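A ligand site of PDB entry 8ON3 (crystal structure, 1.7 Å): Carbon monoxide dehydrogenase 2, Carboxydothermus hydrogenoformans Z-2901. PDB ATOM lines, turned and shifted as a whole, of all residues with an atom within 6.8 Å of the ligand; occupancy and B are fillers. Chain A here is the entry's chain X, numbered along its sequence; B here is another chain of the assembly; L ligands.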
ATOM      1  N   CYS A  47       6.739  14.989   8.020  1.00  0.00           N
ATOM      2  CA  CYS A  47       6.278  13.627   8.229  1.00  0.00           C
ATOM      3  C   CYS A  47       5.611  13.580   9.578  1.00  0.00           C
ATOM      4  O   CYS A  47       6.103  14.192  10.533  1.00  0.00           O
ATOM      5  CB  CYS A  47       7.409  12.600   8.123  1.00  0.00           C
ATOM      6  SG  CYS A  47       6.810  10.917   8.534  1.00  0.00           S
ATOM      7  N   CYS A  48       4.444  12.948   9.631  1.00  0.00           N
ATOM      8  CA  CYS A  48       3.698  12.781  10.877  1.00  0.00           C
ATOM      9  C   CYS A  48       3.269  11.339  11.016  1.00  0.00           C
ATOM     10  O   CYS A  48       2.711  10.751  10.085  1.00  0.00           O
ATOM     11  CB  CYS A  48       2.502  13.741  10.911  1.00  0.00           C
ATOM     12  SG  CYS A  48       1.398  13.516  12.348  1.00  0.00           S
ATOM     13  N   ARG A  49       3.537  10.765  12.188  1.00  0.00           N
ATOM     14  CA  ARG A  49       3.029   9.445  12.535  1.00  0.00           C
ATOM     15  C   ARG A  49       2.227   9.454  13.812  1.00  0.00           C
ATOM     16  O   ARG A  49       2.260   8.470  14.559  1.00  0.00           O
ATOM     17  CB  ARG A  49       4.178   8.460  12.653  1.00  0.00           C
ATOM     18  CG  ARG A  49       4.950   8.250  11.364  1.00  0.00           C
ATOM     19  CD  ARG A  49       6.305   7.597  11.709  1.00  0.00           C
ATOM     20  NE  ARG A  49       6.103   6.293  12.304  1.00  0.00           N
ATOM     21  CZ  ARG A  49       6.996   5.622  13.009  1.00  0.00           C
ATOM     22  NH1 ARG A  49       8.201   6.104  13.239  1.00  0.00           N
ATOM     23  NH2 ARG A  49       6.656   4.444  13.535  1.00  0.00           N
ATOM     24  N   HIS A  50       1.513  10.535  14.085  1.00  0.00           N
ATOM     25  CA  HIS A  50       0.789  10.692  15.324  1.00  0.00           C
ATOM     26  C   HIS A  50      -0.539   9.969  15.364  1.00  0.00           C
ATOM     27  O   HIS A  50      -1.211  10.060  16.377  1.00  0.00           O
ATOM     28  CB  HIS A  50       0.594  12.183  15.620  1.00  0.00           C
ATOM     29  CG  HIS A  50       1.875  12.905  15.916  1.00  0.00           C
ATOM     30  ND1 HIS A  50       1.885  14.136  16.534  1.00  0.00           N
ATOM     31  CD2 HIS A  50       3.162  12.607  15.632  1.00  0.00           C
ATOM     32  CE1 HIS A  50       3.131  14.532  16.688  1.00  0.00           C
ATOM     33  NE2 HIS A  50       3.932  13.630  16.140  1.00  0.00           N
ATOM     34  N   CYS A  51      -0.940   9.245  14.318  1.00  0.00           N
ATOM     35  CA  CYS A  51      -2.052   8.304  14.443  1.00  0.00           C
ATOM     36  C   CYS A  51      -1.845   7.215  13.407  1.00  0.00           C
ATOM     37  O   CYS A  51      -0.929   7.286  12.575  1.00  0.00           O
ATOM     38  CB  CYS A  51      -3.406   8.993  14.298  1.00  0.00           C
ATOM     39  SG  CYS A  51      -3.874   9.306  12.696  1.00  0.00           S
ATOM     40  N   LEU A  52      -2.687   6.181  13.483  1.00  0.00           N
ATOM     41  CA  LEU A  52      -2.561   4.980  12.656  1.00  0.00           C
ATOM     42  C   LEU A  52      -3.175   5.138  11.300  1.00  0.00           C
ATOM     43  O   LEU A  52      -3.248   4.165  10.526  1.00  0.00           O
ATOM     44  CB  LEU A  52      -3.157   3.760  13.360  1.00  0.00           C
ATOM     45  CG  LEU A  52      -2.582   3.377  14.738  1.00  0.00           C
ATOM     46  CD1 LEU A  52      -3.225   2.148  15.361  1.00  0.00           C
ATOM     47  CD2 LEU A  52      -1.092   3.151  14.563  1.00  0.00           C
ATOM     48  N   GLN A  53      -3.637   6.342  10.969  1.00  0.00           N
ATOM     49  CA  GLN A  53      -3.938   6.660   9.609  1.00  0.00           C
ATOM     50  C   GLN A  53      -2.686   6.975   8.820  1.00  0.00           C
ATOM     51  O   GLN A  53      -2.759   6.952   7.586  1.00  0.00           O
ATOM     52  CB  GLN A  53      -4.921   7.823   9.505  1.00  0.00           C
ATOM     53  CG  GLN A  53      -6.294   7.423  10.047  1.00  0.00           C
ATOM     54  CD  GLN A  53      -7.397   8.488   9.857  1.00  0.00           C
ATOM     55  OE1 GLN A  53      -8.552   8.136   9.690  1.00  0.00           O
ATOM     56  NE2 GLN A  53      -7.039   9.770   9.938  1.00  0.00           N
ATOM     57  N   GLY A  54      -1.581   7.283   9.489  1.00  0.00           N
ATOM     58  CA  GLY A  54      -0.353   7.612   8.797  1.00  0.00           C
ATOM     59  C   GLY A  54       0.425   6.358   8.472  1.00  0.00           C
ATOM     60  O   GLY A  54      -0.050   5.226   8.584  1.00  0.00           O
ATOM     61  N   PRO A  55       1.655   6.524   8.090  1.00  0.00           N
ATOM     62  CA  PRO A  55       2.432   7.756   8.071  1.00  0.00           C
ATOM     63  C   PRO A  55       1.889   8.729   7.043  1.00  0.00           C
ATOM     64  O   PRO A  55       1.512   8.344   5.935  1.00  0.00           O
ATOM     65  CB  PRO A  55       3.822   7.257   7.750  1.00  0.00           C
ATOM     66  CG  PRO A  55       3.614   6.052   6.928  1.00  0.00           C
ATOM     67  CD  PRO A  55       2.416   5.394   7.524  1.00  0.00           C
ATOM     68  N   CYS A  56       1.821   9.999   7.416  1.00  0.00           N
ATOM     69  CA  CYS A  56       1.557  11.072   6.476  1.00  0.00           C
ATOM     70  C   CYS A  56       2.837  11.828   6.167  1.00  0.00           C
ATOM     71  O   CYS A  56       3.591  12.182   7.078  1.00  0.00           O
ATOM     72  CB  CYS A  56       0.562  12.045   7.020  1.00  0.00           C
ATOM     73  SG  CYS A  56      -1.037  11.324   7.088  1.00  0.00           S
ATOM     74  N   ARG A  57       3.028  12.141   4.899  1.00  0.00           N
ATOM     75  CA  ARG A  57       4.118  13.002   4.506  1.00  0.00           C
ATOM     76  C   ARG A  57       3.583  14.100   3.598  1.00  0.00           C
ATOM     77  O   ARG A  57       2.496  14.010   3.039  1.00  0.00           O
ATOM     78  CB  ARG A  57       5.226  12.231   3.781  1.00  0.00           C
ATOM     79  CG  ARG A  57       4.817  11.836   2.396  1.00  0.00           C
ATOM     80  CD  ARG A  57       5.490  10.575   1.957  1.00  0.00           C
ATOM     81  NE  ARG A  57       5.103  10.282   0.574  1.00  0.00           N
ATOM     82  CZ  ARG A  57       3.971   9.712   0.200  1.00  0.00           C
ATOM     83  NH1 ARG A  57       3.652   9.589  -1.082  1.00  0.00           N
ATOM     84  NH2 ARG A  57       3.144   9.194   1.123  1.00  0.00           N
ATOM     85  N   VAL A  67      -0.957  17.737   2.128  1.00  0.00           N
ATOM     86  CA  VAL A  67      -1.572  17.949   3.428  1.00  0.00           C
ATOM     87  C   VAL A  67      -1.780  16.602   4.094  1.00  0.00           C
ATOM     88  O   VAL A  67      -1.938  15.583   3.418  1.00  0.00           O
ATOM     89  CB  VAL A  67      -2.906  18.738   3.254  1.00  0.00           C
ATOM     90  CG1 VAL A  67      -3.857  17.954   2.350  1.00  0.00           C
ATOM     91  CG2 VAL A  67      -3.583  19.020   4.599  1.00  0.00           C
ATOM     92  N   GLY A  68      -1.801  16.605   5.418  1.00  0.00           N
ATOM     93  CA  GLY A  68      -2.017  15.381   6.138  1.00  0.00           C
ATOM     94  C   GLY A  68      -3.421  14.839   5.912  1.00  0.00           C
ATOM     95  O   GLY A  68      -4.354  15.552   5.545  1.00  0.00           O
ATOM     96  N   ILE A  69      -3.560  13.534   6.122  1.00  0.00           N
ATOM     97  CA  ILE A  69      -4.871  12.890   5.885  1.00  0.00           C
ATOM     98  C   ILE A  69      -5.982  13.570   6.672  1.00  0.00           C
ATOM     99  O   ILE A  69      -7.108  13.752   6.158  1.00  0.00           O
ATOM    100  CB  ILE A  69      -4.792  11.383   6.239  1.00  0.00           C
ATOM    101  CG1 ILE A  69      -4.004  10.644   5.159  1.00  0.00           C
ATOM    102  CG2 ILE A  69      -6.219  10.800   6.467  1.00  0.00           C
ATOM    103  CD1 ILE A  69      -3.640   9.251   5.566  1.00  0.00           C
ATOM    104  N   CYS A  70      -5.711  13.948   7.928  1.00  0.00           N
ATOM    105  CA  CYS A  70      -6.722  14.566   8.781  1.00  0.00           C
ATOM    106  C   CYS A  70      -6.915  16.048   8.504  1.00  0.00           C
ATOM    107  O   CYS A  70      -7.752  16.689   9.157  1.00  0.00           O
ATOM    108  CB  CYS A  70      -6.361  14.435  10.257  1.00  0.00           C
ATOM    109  SG  CYS A  70      -4.763  15.224  10.623  1.00  0.00           S
ATOM    110  N   GLY A  71      -6.148  16.613   7.547  1.00  0.00           N
ATOM    111  CA  GLY A  71      -6.114  18.032   7.290  1.00  0.00           C
ATOM    112  C   GLY A  71      -4.940  18.764   7.948  1.00  0.00           C
ATOM    113  O   GLY A  71      -4.816  19.980   7.767  1.00  0.00           O
ATOM    114  N   ALA A  72      -4.107  18.087   8.726  1.00  0.00           N
ATOM    115  CA  ALA A  72      -2.939  18.749   9.337  1.00  0.00           C
ATOM    116  C   ALA A  72      -2.049  19.335   8.233  1.00  0.00           C
ATOM    117  O   ALA A  72      -1.504  18.600   7.395  1.00  0.00           O
ATOM    118  CB  ALA A  72      -2.122  17.788  10.198  1.00  0.00           C
ATOM    119  N   THR A  73      -1.858  20.635   8.255  1.00  0.00           N
ATOM    120  CA  THR A  73      -0.979  21.325   7.303  1.00  0.00           C
ATOM    121  C   THR A  73       0.522  21.100   7.612  1.00  0.00           C
ATOM    122  O   THR A  73       0.924  20.577   8.642  1.00  0.00           O
ATOM    123  CB  THR A  73      -1.253  22.829   7.318  1.00  0.00           C
ATOM    124  OG1 THR A  73      -0.931  23.321   8.611  1.00  0.00           O
ATOM    125  CG2 THR A  73      -2.702  23.139   7.001  1.00  0.00           C
ATOM    126  N   ILE A  77       2.165  20.183  11.239  1.00  0.00           N
ATOM    127  CA  ILE A  77       2.949  18.974  11.365  1.00  0.00           C
ATOM    128  C   ILE A  77       4.328  19.330  11.881  1.00  0.00           C
ATOM    129  O   ILE A  77       4.842  18.684  12.816  1.00  0.00           O
ATOM    130  CB  ILE A  77       3.005  18.223  10.022  1.00  0.00           C
ATOM    131  CG1 ILE A  77       1.629  17.603   9.809  1.00  0.00           C
ATOM    132  CG2 ILE A  77       4.146  17.266   9.986  1.00  0.00           C
ATOM    133  CD1 ILE A  77       1.445  16.915   8.485  1.00  0.00           C
ATOM    134  N   ARG A  80       4.185  20.457  15.527  1.00  0.00           N
ATOM    135  CA  ARG A  80       3.900  19.358  16.434  1.00  0.00           C
ATOM    136  C   ARG A  80       5.120  18.497  16.653  1.00  0.00           C
ATOM    137  O   ARG A  80       5.390  18.087  17.798  1.00  0.00           O
ATOM    138  CB  ARG A  80       2.727  18.520  15.915  1.00  0.00           C
ATOM    139  CG  ARG A  80       1.428  19.226  16.018  1.00  0.00           C
ATOM    140  CD  ARG A  80       0.286  18.268  15.816  1.00  0.00           C
ATOM    141  NE  ARG A  80       0.297  17.549  14.550  1.00  0.00           N
ATOM    142  CZ  ARG A  80      -0.778  16.975  14.022  1.00  0.00           C
ATOM    143  NH1 ARG A  80      -1.947  17.000  14.634  1.00  0.00           N
ATOM    144  NH2 ARG A  80      -0.672  16.336  12.862  1.00  0.00           N
ATOM    145  N   THR A 197      -0.317  17.962  20.850  1.00  0.00           N
ATOM    146  CA  THR A 197       0.243  17.523  19.580  1.00  0.00           C
ATOM    147  C   THR A 197      -0.342  16.209  19.083  1.00  0.00           C
ATOM    148  O   THR A 197      -0.058  15.811  17.956  1.00  0.00           O
ATOM    149  CB  THR A 197       1.775  17.389  19.664  1.00  0.00           C
ATOM    150  OG1 THR A 197       2.109  16.463  20.700  1.00  0.00           O
ATOM    151  CG2 THR A 197       2.439  18.730  19.983  1.00  0.00           C
ATOM    152  N   SER A 198      -1.202  15.544  19.865  1.00  0.00           N
ATOM    153  CA  SER A 198      -1.823  14.301  19.438  1.00  0.00           C
ATOM    154  C   SER A 198      -2.875  14.636  18.391  1.00  0.00           C
ATOM    155  O   SER A 198      -3.192  15.806  18.171  1.00  0.00           O
ATOM    156  CB  SER A 198      -2.406  13.555  20.642  1.00  0.00           C
ATOM    157  OG  SER A 198      -3.579  14.209  21.076  1.00  0.00           O
ATOM    158  N   MET A 199      -3.360  13.612  17.659  1.00  0.00           N
ATOM    159  CA  MET A 199      -4.194  13.870  16.496  1.00  0.00           C
ATOM    160  C   MET A 199      -5.468  14.602  16.892  1.00  0.00           C
ATOM    161  O   MET A 199      -6.097  14.315  17.917  1.00  0.00           O
ATOM    162  CB  MET A 199      -4.544  12.568  15.772  1.00  0.00           C
ATOM    163  CG  MET A 199      -5.500  12.700  14.561  1.00  0.00           C
ATOM    164  SD  MET A 199      -7.226  12.769  15.048  1.00  0.00           S
ATOM    165  CE  MET A 199      -8.034  13.262  13.554  1.00  0.00           C
ATOM    166  N   GLY A 200      -5.826  15.566  16.062  1.00  0.00           N
ATOM    167  CA  GLY A 200      -7.063  16.265  16.253  1.00  0.00           C
ATOM    168  C   GLY A 200      -7.126  17.210  17.424  1.00  0.00           C
ATOM    169  O   GLY A 200      -8.220  17.445  17.951  1.00  0.00           O
ATOM    170  N   MET B  35      -2.250  10.449  -0.423  1.00  0.00           N
ATOM    171  CA  MET B  35      -1.100  10.006   0.335  1.00  0.00           C
ATOM    172  C   MET B  35      -0.582   8.630  -0.099  1.00  0.00           C
ATOM    173  O   MET B  35       0.469   8.213   0.391  1.00  0.00           O
ATOM    174  CB  MET B  35      -1.484   9.973   1.823  1.00  0.00           C
ATOM    175  CG  MET B  35      -0.350   9.903   2.805  1.00  0.00           C
ATOM    176  SD  MET B  35       0.640  11.392   2.728  1.00  0.00           S
ATOM    177  CE  MET B  35      -0.515  12.577   3.431  1.00  0.00           C
ATOM    178  N   GLN B  38       1.668   4.923   1.083  1.00  0.00           N
ATOM    179  CA  GLN B  38       2.234   5.477   2.307  1.00  0.00           C
ATOM    180  C   GLN B  38       3.584   4.839   2.575  1.00  0.00           C
ATOM    181  O   GLN B  38       3.948   3.792   2.013  1.00  0.00           O
ATOM    182  CB  GLN B  38       1.303   5.257   3.485  1.00  0.00           C
ATOM    183  CG  GLN B  38       0.042   6.053   3.304  1.00  0.00           C
ATOM    184  CD  GLN B  38      -0.941   5.836   4.397  1.00  0.00           C
ATOM    185  OE1 GLN B  38      -1.728   4.916   4.353  1.00  0.00           O
ATOM    186  NE2 GLN B  38      -0.898   6.697   5.400  1.00  0.00           N
ATOM    187  N   PRO B 336      -8.598  18.883  11.544  1.00  0.00           N
ATOM    188  CA  PRO B 336      -8.422  20.330  11.350  1.00  0.00           C
ATOM    189  C   PRO B 336      -8.869  20.811   9.996  1.00  0.00           C
ATOM    190  O   PRO B 336      -9.089  22.020   9.850  1.00  0.00           O
ATOM    191  CB  PRO B 336      -6.915  20.539  11.570  1.00  0.00           C
ATOM    192  CG  PRO B 336      -6.313  19.174  11.360  1.00  0.00           C
ATOM    193  CD  PRO B 336      -7.315  18.247  11.923  1.00  0.00           C
ATOM    194  N   MET B 560      -7.352   4.275  15.476  1.00  0.00           N
ATOM    195  CA  MET B 560      -6.734   5.422  14.815  1.00  0.00           C
ATOM    196  C   MET B 560      -5.830   6.170  15.781  1.00  0.00           C
ATOM    197  O   MET B 560      -4.626   6.299  15.538  1.00  0.00           O
ATOM    198  CB  MET B 560      -7.810   6.357  14.241  1.00  0.00           C
ATOM    199  CG  MET B 560      -7.332   7.611  13.527  1.00  0.00           C
ATOM    200  SD  MET B 560      -7.131   9.099  14.523  1.00  0.00           S
ATOM    201  CE  MET B 560      -8.845   9.443  14.928  1.00  0.00           C
HETATM  202 FE1  LIG L   1      -1.672  11.823   9.312  1.00  0.00          FE
HETATM  203 FE2  LIG L   1      -3.073  13.591  10.814  1.00  0.00          FE
HETATM  204 FE3  LIG L   1      -0.579  12.786  11.524  1.00  0.00          FE
HETATM  205 FE4  LIG L   1      -2.581  11.030  11.685  1.00  0.00          FE
HETATM  206  S1  LIG L   1      -2.289  12.953  12.913  1.00  0.00           S
HETATM  207  S2  LIG L   1      -0.581  10.626  10.860  1.00  0.00           S
HETATM  208  S3  LIG L   1      -3.826  11.681   9.844  1.00  0.00           S
HETATM  209  S4  LIG L   1      -1.207  14.070   9.716  1.00  0.00           S
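Merely in contact with the ligand: Met 199, Ile 69, His 50, Ala 72 and Gly 68. Hydrophobic or aromatic side chains that line the ligand: Ile 69, Ala 72 and Met 199. Of the 28 residues printed, 12 come within 4 Å of the ligand. The nearest printed residue that does not touch the ligand is Ile 77 (4.1 Å).
FE3 of the ligand is bound by SG of Cys 48, at 2.3 Å. The backbone NH of Cys 70 sits close to a sulfur (S3) of the ligand, at 3.5 Å. An iron atom (FE2) of the ligand is bound by the side-chain sulfur of Cys 70. FE1 of the ligand is bound by SG of Cys 56 (2.4 Å). N of Cys 51 lies close to S2 of the ligand, 3.7 Å away. FE4 of the ligand is bound by SG of Cys 51 (2.4 Å). The backbone NH (N) of Gly 54 lies close to a sulfur (S2) of the ligand (3.7 Å). The side-chain amide nitrogen (NE2) of Gln 53 sits close to a sulfur (S3) of the ligand. NH2 of Arg 80 lies close to S1 of the ligand, 3.7 Å away.
The backbone NH (N) of Cys 48 lies within hydrogen-bond range of the backbone carbonyl oxygen (O) of Cys 56. The side-chain sulfur of Cys 48 lies close to the guanidinium group of Arg 80, 3.5 Å away. The backbone NH (N) of His 50 sits close to the side-chain sulfur (SG) of Cys 48, 3.5 Å away. The backbone NH (N) of Ile 69 sits close to the side-chain sulfur (SG) of Cys 56 (3.5 Å). SG of Cys 47 sits close to O of Cys 56. SG of Cys 51 sits close to N of Gln 53 (3.4 Å). SG of Cys 51 lies close to SD of Met 560 of chain B. NE2 of Gln 38 of chain B is in hydrogen-bond range of O of Gln 53 (2.9 Å).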
